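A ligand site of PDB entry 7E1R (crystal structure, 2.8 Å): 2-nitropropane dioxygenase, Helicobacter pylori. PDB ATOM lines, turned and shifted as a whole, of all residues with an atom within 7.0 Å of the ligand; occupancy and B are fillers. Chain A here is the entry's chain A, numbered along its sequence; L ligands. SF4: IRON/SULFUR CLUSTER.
N of Cys 317 is in hydrogen-bond range of O of Pro 283 (3.5 Å).
The side-chain amino group of Lys 324 lies close to the backbone carbonyl oxygen of Gly 320 (3.3 Å).
The backbone carbonyl oxygen (O) of Cys 313 sits at hydrogen-bond distance from the backbone NH (N) of Asn 114.
The side-chain sulfur of Cys 329 sits close to the backbone NH of Asp 332 (3.1 Å).
N of Ala 331 lies close to SG of Cys 329 (3.5 Å).
O of Asn 312 is in hydrogen-bond range of ND2 of Asn 114 (3.1 Å).
The backbone carbonyl oxygen (O) of Cys 317 lies within hydrogen-bond range of the backbone NH (N) of Glu 322 (3.1 Å).
The backbone NH (N) of Asn 312 sits close to the side-chain sulfur (SG) of Cys 309, at 3.8 Å.
N of Gly 320 sits close to S4 of the ligand, 3.6 Å away.
The backbone NH of Cys 313 sits close to a sulfur (S3) of the ligand (3.6 Å).
S2 of the ligand lies close to N of Asn 312, at 3.4 Å.
SG of Cys 329 is bound to FE3 of the ligand (2.5 Å).
SG of Cys 313 is bound to FE4 of the ligand (2.6 Å).
The backbone NH (N) of Ile 330 sits close to a sulfur (S1) of the ligand, 3.4 Å away.
The side-chain sulfur (SG) of Cys 309 is bound to an iron atom (FE1) of the ligand (2.6 Å).
FE2 of the ligand is bound by SG of Cys 317, at 2.6 Å.
O of Val 314 sits close to S3 of the ligand, at 3.8 Å.
CB of Ser 311 touches S2 of the ligand (3.997 Å).
CB of Ala 323 touches S4 of the ligand, at 3.8 Å.
Ala 331 touches the ligand.
Within 4 Å of the ligand: Cys 309, Ser 311, Asn 312, Cys 313, Val 314, Cys 317, Gly 320, Ala 323, Cys 329, Ile 330 and Ala 331.
Along chain A the residues within 4 Å of the ligand span positions 309 to 331.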
ATOM      1  N   PHE A  83      29.736   8.475  24.633  1.00  0.00           N
ATOM      2  CA  PHE A  83      30.035   9.545  23.689  1.00  0.00           C
ATOM      3  C   PHE A  83      31.540   9.677  23.504  1.00  0.00           C
ATOM      4  O   PHE A  83      32.028   9.854  22.372  1.00  0.00           O
ATOM      5  CB  PHE A  83      29.421  10.846  24.174  1.00  0.00           C
ATOM      6  CG  PHE A  83      29.544  11.981  23.197  1.00  0.00           C
ATOM      7  CD1 PHE A  83      28.742  12.015  22.068  1.00  0.00           C
ATOM      8  CD2 PHE A  83      30.440  13.007  23.427  1.00  0.00           C
ATOM      9  CE1 PHE A  83      28.856  13.065  21.164  1.00  0.00           C
ATOM     10  CE2 PHE A  83      30.561  14.055  22.530  1.00  0.00           C
ATOM     11  CZ  PHE A  83      29.758  14.090  21.401  1.00  0.00           C
ATOM     12  N   ASN A 114      32.038  16.991  29.872  1.00  0.00           N
ATOM     13  CA  ASN A 114      31.985  16.118  31.033  1.00  0.00           C
ATOM     14  C   ASN A 114      33.042  15.028  30.919  1.00  0.00           C
ATOM     15  O   ASN A 114      33.400  14.598  29.820  1.00  0.00           O
ATOM     16  CB  ASN A 114      30.592  15.501  31.154  1.00  0.00           C
ATOM     17  CG  ASN A 114      29.593  16.480  31.717  1.00  0.00           C
ATOM     18  OD1 ASN A 114      29.908  17.252  32.619  1.00  0.00           O
ATOM     19  ND2 ASN A 114      28.380  16.467  31.168  1.00  0.00           N
ATOM     20  N   PRO A 283      25.307  25.418  22.917  1.00  0.00           N
ATOM     21  CA  PRO A 283      25.136  24.967  24.314  1.00  0.00           C
ATOM     22  C   PRO A 283      26.427  24.986  25.109  1.00  0.00           C
ATOM     23  O   PRO A 283      26.384  24.901  26.341  1.00  0.00           O
ATOM     24  CB  PRO A 283      24.590  23.537  24.179  1.00  0.00           C
ATOM     25  CG  PRO A 283      24.254  23.364  22.724  1.00  0.00           C
ATOM     26  CD  PRO A 283      25.148  24.297  21.975  1.00  0.00           C
ATOM     27  N   VAL A 284      27.581  25.090  24.442  1.00  0.00           N
ATOM     28  CA  VAL A 284      28.868  25.148  25.118  1.00  0.00           C
ATOM     29  C   VAL A 284      29.115  26.520  25.733  1.00  0.00           C
ATOM     30  O   VAL A 284      29.944  26.653  26.634  1.00  0.00           O
ATOM     31  CB  VAL A 284      30.002  24.776  24.137  1.00  0.00           C
ATOM     32  CG1 VAL A 284      31.301  24.528  24.864  1.00  0.00           C
ATOM     33  CG2 VAL A 284      29.632  23.548  23.331  1.00  0.00           C
ATOM     34  N   ILE A 307      14.928  17.613  20.955  1.00  0.00           N
ATOM     35  CA  ILE A 307      16.085  17.614  21.839  1.00  0.00           C
ATOM     36  C   ILE A 307      15.790  16.677  23.000  1.00  0.00           C
ATOM     37  O   ILE A 307      14.793  16.840  23.720  1.00  0.00           O
ATOM     38  CB  ILE A 307      16.430  19.030  22.319  1.00  0.00           C
ATOM     39  CG1 ILE A 307      17.246  19.762  21.260  1.00  0.00           C
ATOM     40  CG2 ILE A 307      17.235  18.984  23.597  1.00  0.00           C
ATOM     41  CD1 ILE A 307      16.930  21.233  21.116  1.00  0.00           C
ATOM     42  N   ALA A 308      16.666  15.696  23.207  1.00  0.00           N
ATOM     43  CA  ALA A 308      16.549  14.770  24.335  1.00  0.00           C
ATOM     44  C   ALA A 308      17.975  14.400  24.705  1.00  0.00           C
ATOM     45  O   ALA A 308      18.604  13.598  24.007  1.00  0.00           O
ATOM     46  CB  ALA A 308      15.732  13.538  23.965  1.00  0.00           C
ATOM     47  N   CYS A 309      18.471  14.972  25.809  1.00  0.00           N
ATOM     48  CA  CYS A 309      19.872  14.807  26.163  1.00  0.00           C
ATOM     49  C   CYS A 309      20.228  13.346  26.405  1.00  0.00           C
ATOM     50  O   CYS A 309      19.905  12.791  27.461  1.00  0.00           O
ATOM     51  CB  CYS A 309      20.209  15.651  27.401  1.00  0.00           C
ATOM     52  SG  CYS A 309      21.901  15.448  27.982  1.00  0.00           S
ATOM     53  N   VAL A 310      20.842  12.708  25.410  1.00  0.00           N
ATOM     54  CA  VAL A 310      21.325  11.346  25.554  1.00  0.00           C
ATOM     55  C   VAL A 310      22.833  11.283  25.799  1.00  0.00           C
ATOM     56  O   VAL A 310      23.298  10.549  26.665  1.00  0.00           O
ATOM     57  CB  VAL A 310      20.933  10.517  24.309  1.00  0.00           C
ATOM     58  CG1 VAL A 310      21.550   9.131  24.383  1.00  0.00           C
ATOM     59  CG2 VAL A 310      19.421  10.441  24.175  1.00  0.00           C
ATOM     60  N   SER A 311      23.624  12.035  25.017  1.00  0.00           N
ATOM     61  CA  SER A 311      25.078  11.895  25.129  1.00  0.00           C
ATOM     62  C   SER A 311      25.695  12.697  26.272  1.00  0.00           C
ATOM     63  O   SER A 311      26.781  12.333  26.742  1.00  0.00           O
ATOM     64  CB  SER A 311      25.737  12.306  23.806  1.00  0.00           C
ATOM     65  OG  SER A 311      25.504  11.369  22.767  1.00  0.00           O
ATOM     66  N   ASN A 312      25.026  13.751  26.754  1.00  0.00           N
ATOM     67  CA  ASN A 312      25.509  14.572  27.888  1.00  0.00           C
ATOM     68  C   ASN A 312      26.940  15.093  27.686  1.00  0.00           C
ATOM     69  O   ASN A 312      27.809  14.935  28.543  1.00  0.00           O
ATOM     70  CB  ASN A 312      25.360  13.805  29.201  1.00  0.00           C
ATOM     71  CG  ASN A 312      25.461  14.707  30.414  1.00  0.00           C
ATOM     72  OD1 ASN A 312      25.172  15.909  30.340  1.00  0.00           O
ATOM     73  ND2 ASN A 312      25.783  14.112  31.549  1.00  0.00           N
ATOM     74  N   CYS A 313      27.173  15.711  26.530  1.00  0.00           N
ATOM     75  CA  CYS A 313      28.540  15.916  26.055  1.00  0.00           C
ATOM     76  C   CYS A 313      29.300  16.988  26.842  1.00  0.00           C
ATOM     77  O   CYS A 313      30.509  16.825  27.078  1.00  0.00           O
ATOM     78  CB  CYS A 313      28.540  16.235  24.570  1.00  0.00           C
ATOM     79  SG  CYS A 313      27.882  17.823  24.133  1.00  0.00           S
ATOM     80  N   VAL A 314      28.653  18.097  27.238  1.00  0.00           N
ATOM     81  CA  VAL A 314      29.380  19.238  27.818  1.00  0.00           C
ATOM     82  C   VAL A 314      28.683  19.708  29.085  1.00  0.00           C
ATOM     83  O   VAL A 314      27.450  19.716  29.178  1.00  0.00           O
ATOM     84  CB  VAL A 314      29.535  20.440  26.851  1.00  0.00           C
ATOM     85  CG1 VAL A 314      30.481  20.124  25.692  1.00  0.00           C
ATOM     86  CG2 VAL A 314      28.218  21.017  26.423  1.00  0.00           C
ATOM     87  N   ALA A 315      29.492  20.087  30.072  1.00  0.00           N
ATOM     88  CA  ALA A 315      28.956  20.587  31.332  1.00  0.00           C
ATOM     89  C   ALA A 315      28.134  21.869  31.225  1.00  0.00           C
ATOM     90  O   ALA A 315      27.076  21.941  31.866  1.00  0.00           O
ATOM     91  CB  ALA A 315      30.116  20.781  32.316  1.00  0.00           C
ATOM     92  N   PRO A 316      28.544  22.906  30.471  1.00  0.00           N
ATOM     93  CA  PRO A 316      27.774  24.162  30.511  1.00  0.00           C
ATOM     94  C   PRO A 316      26.341  24.060  30.007  1.00  0.00           C
ATOM     95  O   PRO A 316      25.521  24.913  30.362  1.00  0.00           O
ATOM     96  CB  PRO A 316      28.600  25.092  29.611  1.00  0.00           C
ATOM     97  CG  PRO A 316      29.975  24.523  29.625  1.00  0.00           C
ATOM     98  CD  PRO A 316      29.780  23.044  29.682  1.00  0.00           C
ATOM     99  N   CYS A 317      25.995  23.028  29.247  1.00  0.00           N
ATOM    100  CA  CYS A 317      24.629  22.932  28.730  1.00  0.00           C
ATOM    101  C   CYS A 317      23.631  22.525  29.795  1.00  0.00           C
ATOM    102  O   CYS A 317      22.448  22.856  29.689  1.00  0.00           O
ATOM    103  CB  CYS A 317      24.579  21.985  27.534  1.00  0.00           C
ATOM    104  SG  CYS A 317      22.918  21.706  26.917  1.00  0.00           S
ATOM    105  N   ASN A 318      24.091  21.846  30.850  1.00  0.00           N
ATOM    106  CA  ASN A 318      23.229  21.397  31.944  1.00  0.00           C
ATOM    107  C   ASN A 318      22.163  20.391  31.480  1.00  0.00           C
ATOM    108  O   ASN A 318      20.979  20.519  31.780  1.00  0.00           O
ATOM    109  CB  ASN A 318      22.590  22.579  32.674  1.00  0.00           C
ATOM    110  CG  ASN A 318      23.520  23.198  33.702  1.00  0.00           C
ATOM    111  OD1 ASN A 318      24.131  22.488  34.509  1.00  0.00           O
ATOM    112  ND2 ASN A 318      23.650  24.528  33.676  1.00  0.00           N
ATOM    113  N   ARG A 319      22.556  19.517  30.625  1.00  0.00           N
ATOM    114  CA  ARG A 319      21.746  18.465  30.261  1.00  0.00           C
ATOM    115  C   ARG A 319      20.611  18.583  29.389  1.00  0.00           C
ATOM    116  O   ARG A 319      19.672  17.837  29.459  1.00  0.00           O
ATOM    117  CB  ARG A 319      21.406  17.788  31.492  1.00  0.00           C
ATOM    118  CG  ARG A 319      22.295  16.679  31.635  1.00  0.00           C
ATOM    119  CD  ARG A 319      21.950  16.042  32.875  1.00  0.00           C
ATOM    120  NE  ARG A 319      22.237  16.945  33.919  1.00  0.00           N
ATOM    121  CZ  ARG A 319      21.368  17.494  34.718  1.00  0.00           C
ATOM    122  NH1 ARG A 319      20.112  17.248  34.605  1.00  0.00           N
ATOM    123  NH2 ARG A 319      21.799  18.298  35.623  1.00  0.00           N
ATOM    124  N   GLY A 320      20.756  19.497  28.507  1.00  0.00           N
ATOM    125  CA  GLY A 320      19.769  19.827  27.496  1.00  0.00           C
ATOM    126  C   GLY A 320      19.093  21.165  27.690  1.00  0.00           C
ATOM    127  O   GLY A 320      18.366  21.618  26.800  1.00  0.00           O
ATOM    128  N   GLU A 321      19.360  21.785  28.776  1.00  0.00           N
ATOM    129  CA  GLU A 321      18.756  23.014  29.014  1.00  0.00           C
ATOM    130  C   GLU A 321      19.165  24.035  28.080  1.00  0.00           C
ATOM    131  O   GLU A 321      18.406  24.662  27.556  1.00  0.00           O
ATOM    132  CB  GLU A 321      19.147  23.486  30.326  1.00  0.00           C
ATOM    133  CG  GLU A 321      18.270  23.028  31.418  1.00  0.00           C
ATOM    134  CD  GLU A 321      18.713  23.588  32.715  1.00  0.00           C
ATOM    135  OE1 GLU A 321      19.145  24.724  32.721  1.00  0.00           O
ATOM    136  OE2 GLU A 321      18.645  22.901  33.708  1.00  0.00           O
ATOM    137  N   GLU A 322      20.417  24.286  27.879  1.00  0.00           N
ATOM    138  CA  GLU A 322      20.855  25.277  26.919  1.00  0.00           C
ATOM    139  C   GLU A 322      20.767  24.859  25.556  1.00  0.00           C
ATOM    140  O   GLU A 322      20.788  25.638  24.714  1.00  0.00           O
ATOM    141  CB  GLU A 322      22.214  25.767  27.163  1.00  0.00           C
ATOM    142  CG  GLU A 322      22.476  25.867  28.590  1.00  0.00           C
ATOM    143  CD  GLU A 322      22.011  27.121  29.169  1.00  0.00           C
ATOM    144  OE1 GLU A 322      21.973  28.079  28.524  1.00  0.00           O
ATOM    145  OE2 GLU A 322      21.716  27.121  30.303  1.00  0.00           O
ATOM    146  N   ALA A 323      20.781  23.589  25.326  1.00  0.00           N
ATOM    147  CA  ALA A 323      20.457  23.114  23.986  1.00  0.00           C
ATOM    148  C   ALA A 323      19.039  23.555  23.593  1.00  0.00           C
ATOM    149  O   ALA A 323      18.823  24.090  22.495  1.00  0.00           O
ATOM    150  CB  ALA A 323      20.602  21.591  23.926  1.00  0.00           C
ATOM    151  N   LYS A 324      18.082  23.571  24.479  1.00  0.00           N
ATOM    152  CA  LYS A 324      16.781  23.949  24.140  1.00  0.00           C
ATOM    153  C   LYS A 324      16.716  25.377  24.075  1.00  0.00           C
ATOM    154  O   LYS A 324      16.018  25.915  23.352  1.00  0.00           O
ATOM    155  CB  LYS A 324      15.836  23.450  25.177  1.00  0.00           C
ATOM    156  CG  LYS A 324      15.781  21.951  25.364  1.00  0.00           C
ATOM    157  CD  LYS A 324      14.689  21.548  26.325  1.00  0.00           C
ATOM    158  CE  LYS A 324      14.635  20.102  26.595  1.00  0.00           C
ATOM    159  NZ  LYS A 324      15.721  19.870  27.554  1.00  0.00           N
ATOM    160  N   TYR A 328      19.199  23.434  19.403  1.00  0.00           N
ATOM    161  CA  TYR A 328      19.804  22.218  18.873  1.00  0.00           C
ATOM    162  C   TYR A 328      20.770  21.619  19.876  1.00  0.00           C
ATOM    163  O   TYR A 328      21.300  22.286  20.762  1.00  0.00           O
ATOM    164  CB  TYR A 328      20.511  22.515  17.548  1.00  0.00           C
ATOM    165  CG  TYR A 328      21.728  23.382  17.736  1.00  0.00           C
ATOM    166  CD1 TYR A 328      21.604  24.765  17.775  1.00  0.00           C
ATOM    167  CD2 TYR A 328      22.995  22.830  17.887  1.00  0.00           C
ATOM    168  CE1 TYR A 328      22.695  25.579  17.964  1.00  0.00           C
ATOM    169  CE2 TYR A 328      24.102  23.644  18.065  1.00  0.00           C
ATOM    170  CZ  TYR A 328      23.955  25.018  18.107  1.00  0.00           C
ATOM    171  OH  TYR A 328      25.042  25.835  18.275  1.00  0.00           O
ATOM    172  N   CYS A 329      20.984  20.322  19.690  1.00  0.00           N
ATOM    173  CA  CYS A 329      21.950  19.560  20.468  1.00  0.00           C
ATOM    174  C   CYS A 329      23.223  19.386  19.646  1.00  0.00           C
ATOM    175  O   CYS A 329      23.183  18.916  18.507  1.00  0.00           O
ATOM    176  CB  CYS A 329      21.357  18.205  20.825  1.00  0.00           C
ATOM    177  SG  CYS A 329      22.594  17.012  21.221  1.00  0.00           S
ATOM    178  N   ILE A 330      24.352  19.816  20.214  1.00  0.00           N
ATOM    179  CA  ILE A 330      25.562  19.857  19.406  1.00  0.00           C
ATOM    180  C   ILE A 330      26.142  18.461  19.254  1.00  0.00           C
ATOM    181  O   ILE A 330      26.730  18.132  18.205  1.00  0.00           O
ATOM    182  CB  ILE A 330      26.563  20.844  20.033  1.00  0.00           C
ATOM    183  CG1 ILE A 330      27.681  21.176  19.056  1.00  0.00           C
ATOM    184  CG2 ILE A 330      27.135  20.310  21.326  1.00  0.00           C
ATOM    185  CD1 ILE A 330      28.626  22.257  19.560  1.00  0.00           C
ATOM    186  N   ALA A 331      25.918  17.585  20.228  1.00  0.00           N
ATOM    187  CA  ALA A 331      26.369  16.198  20.088  1.00  0.00           C
ATOM    188  C   ALA A 331      25.598  15.493  18.989  1.00  0.00           C
ATOM    189  O   ALA A 331      26.190  14.891  18.079  1.00  0.00           O
ATOM    190  CB  ALA A 331      26.213  15.469  21.424  1.00  0.00           C
ATOM    191  N   ASP A 332      24.267  15.646  18.987  1.00  0.00           N
ATOM    192  CA  ASP A 332      23.452  15.021  17.945  1.00  0.00           C
ATOM    193  C   ASP A 332      23.779  15.619  16.586  1.00  0.00           C
ATOM    194  O   ASP A 332      23.954  14.879  15.613  1.00  0.00           O
ATOM    195  CB  ASP A 332      21.955  15.180  18.251  1.00  0.00           C
ATOM    196  CG  ASP A 332      21.527  14.484  19.548  1.00  0.00           C
ATOM    197  OD1 ASP A 332      22.359  13.792  20.185  1.00  0.00           O
ATOM    198  OD2 ASP A 332      20.347  14.615  19.935  1.00  0.00           O
HETATM  199 FE1  SF4 L   1      23.162  16.852  26.170  1.00  0.00          FE
HETATM  200 FE2  SF4 L   1      23.437  19.510  25.635  1.00  0.00          FE
HETATM  201 FE3  SF4 L   1      23.006  17.770  23.599  1.00  0.00          FE
HETATM  202 FE4  SF4 L   1      25.383  17.765  24.896  1.00  0.00          FE
HETATM  203  S1  SF4 L   1      24.506  19.463  23.639  1.00  0.00           S
HETATM  204  S2  SF4 L   1      24.165  15.942  24.340  1.00  0.00           S
HETATM  205  S3  SF4 L   1      24.742  18.254  27.013  1.00  0.00           S
HETATM  206  S4  SF4 L   1      21.592  18.236  25.295  1.00  0.00           S
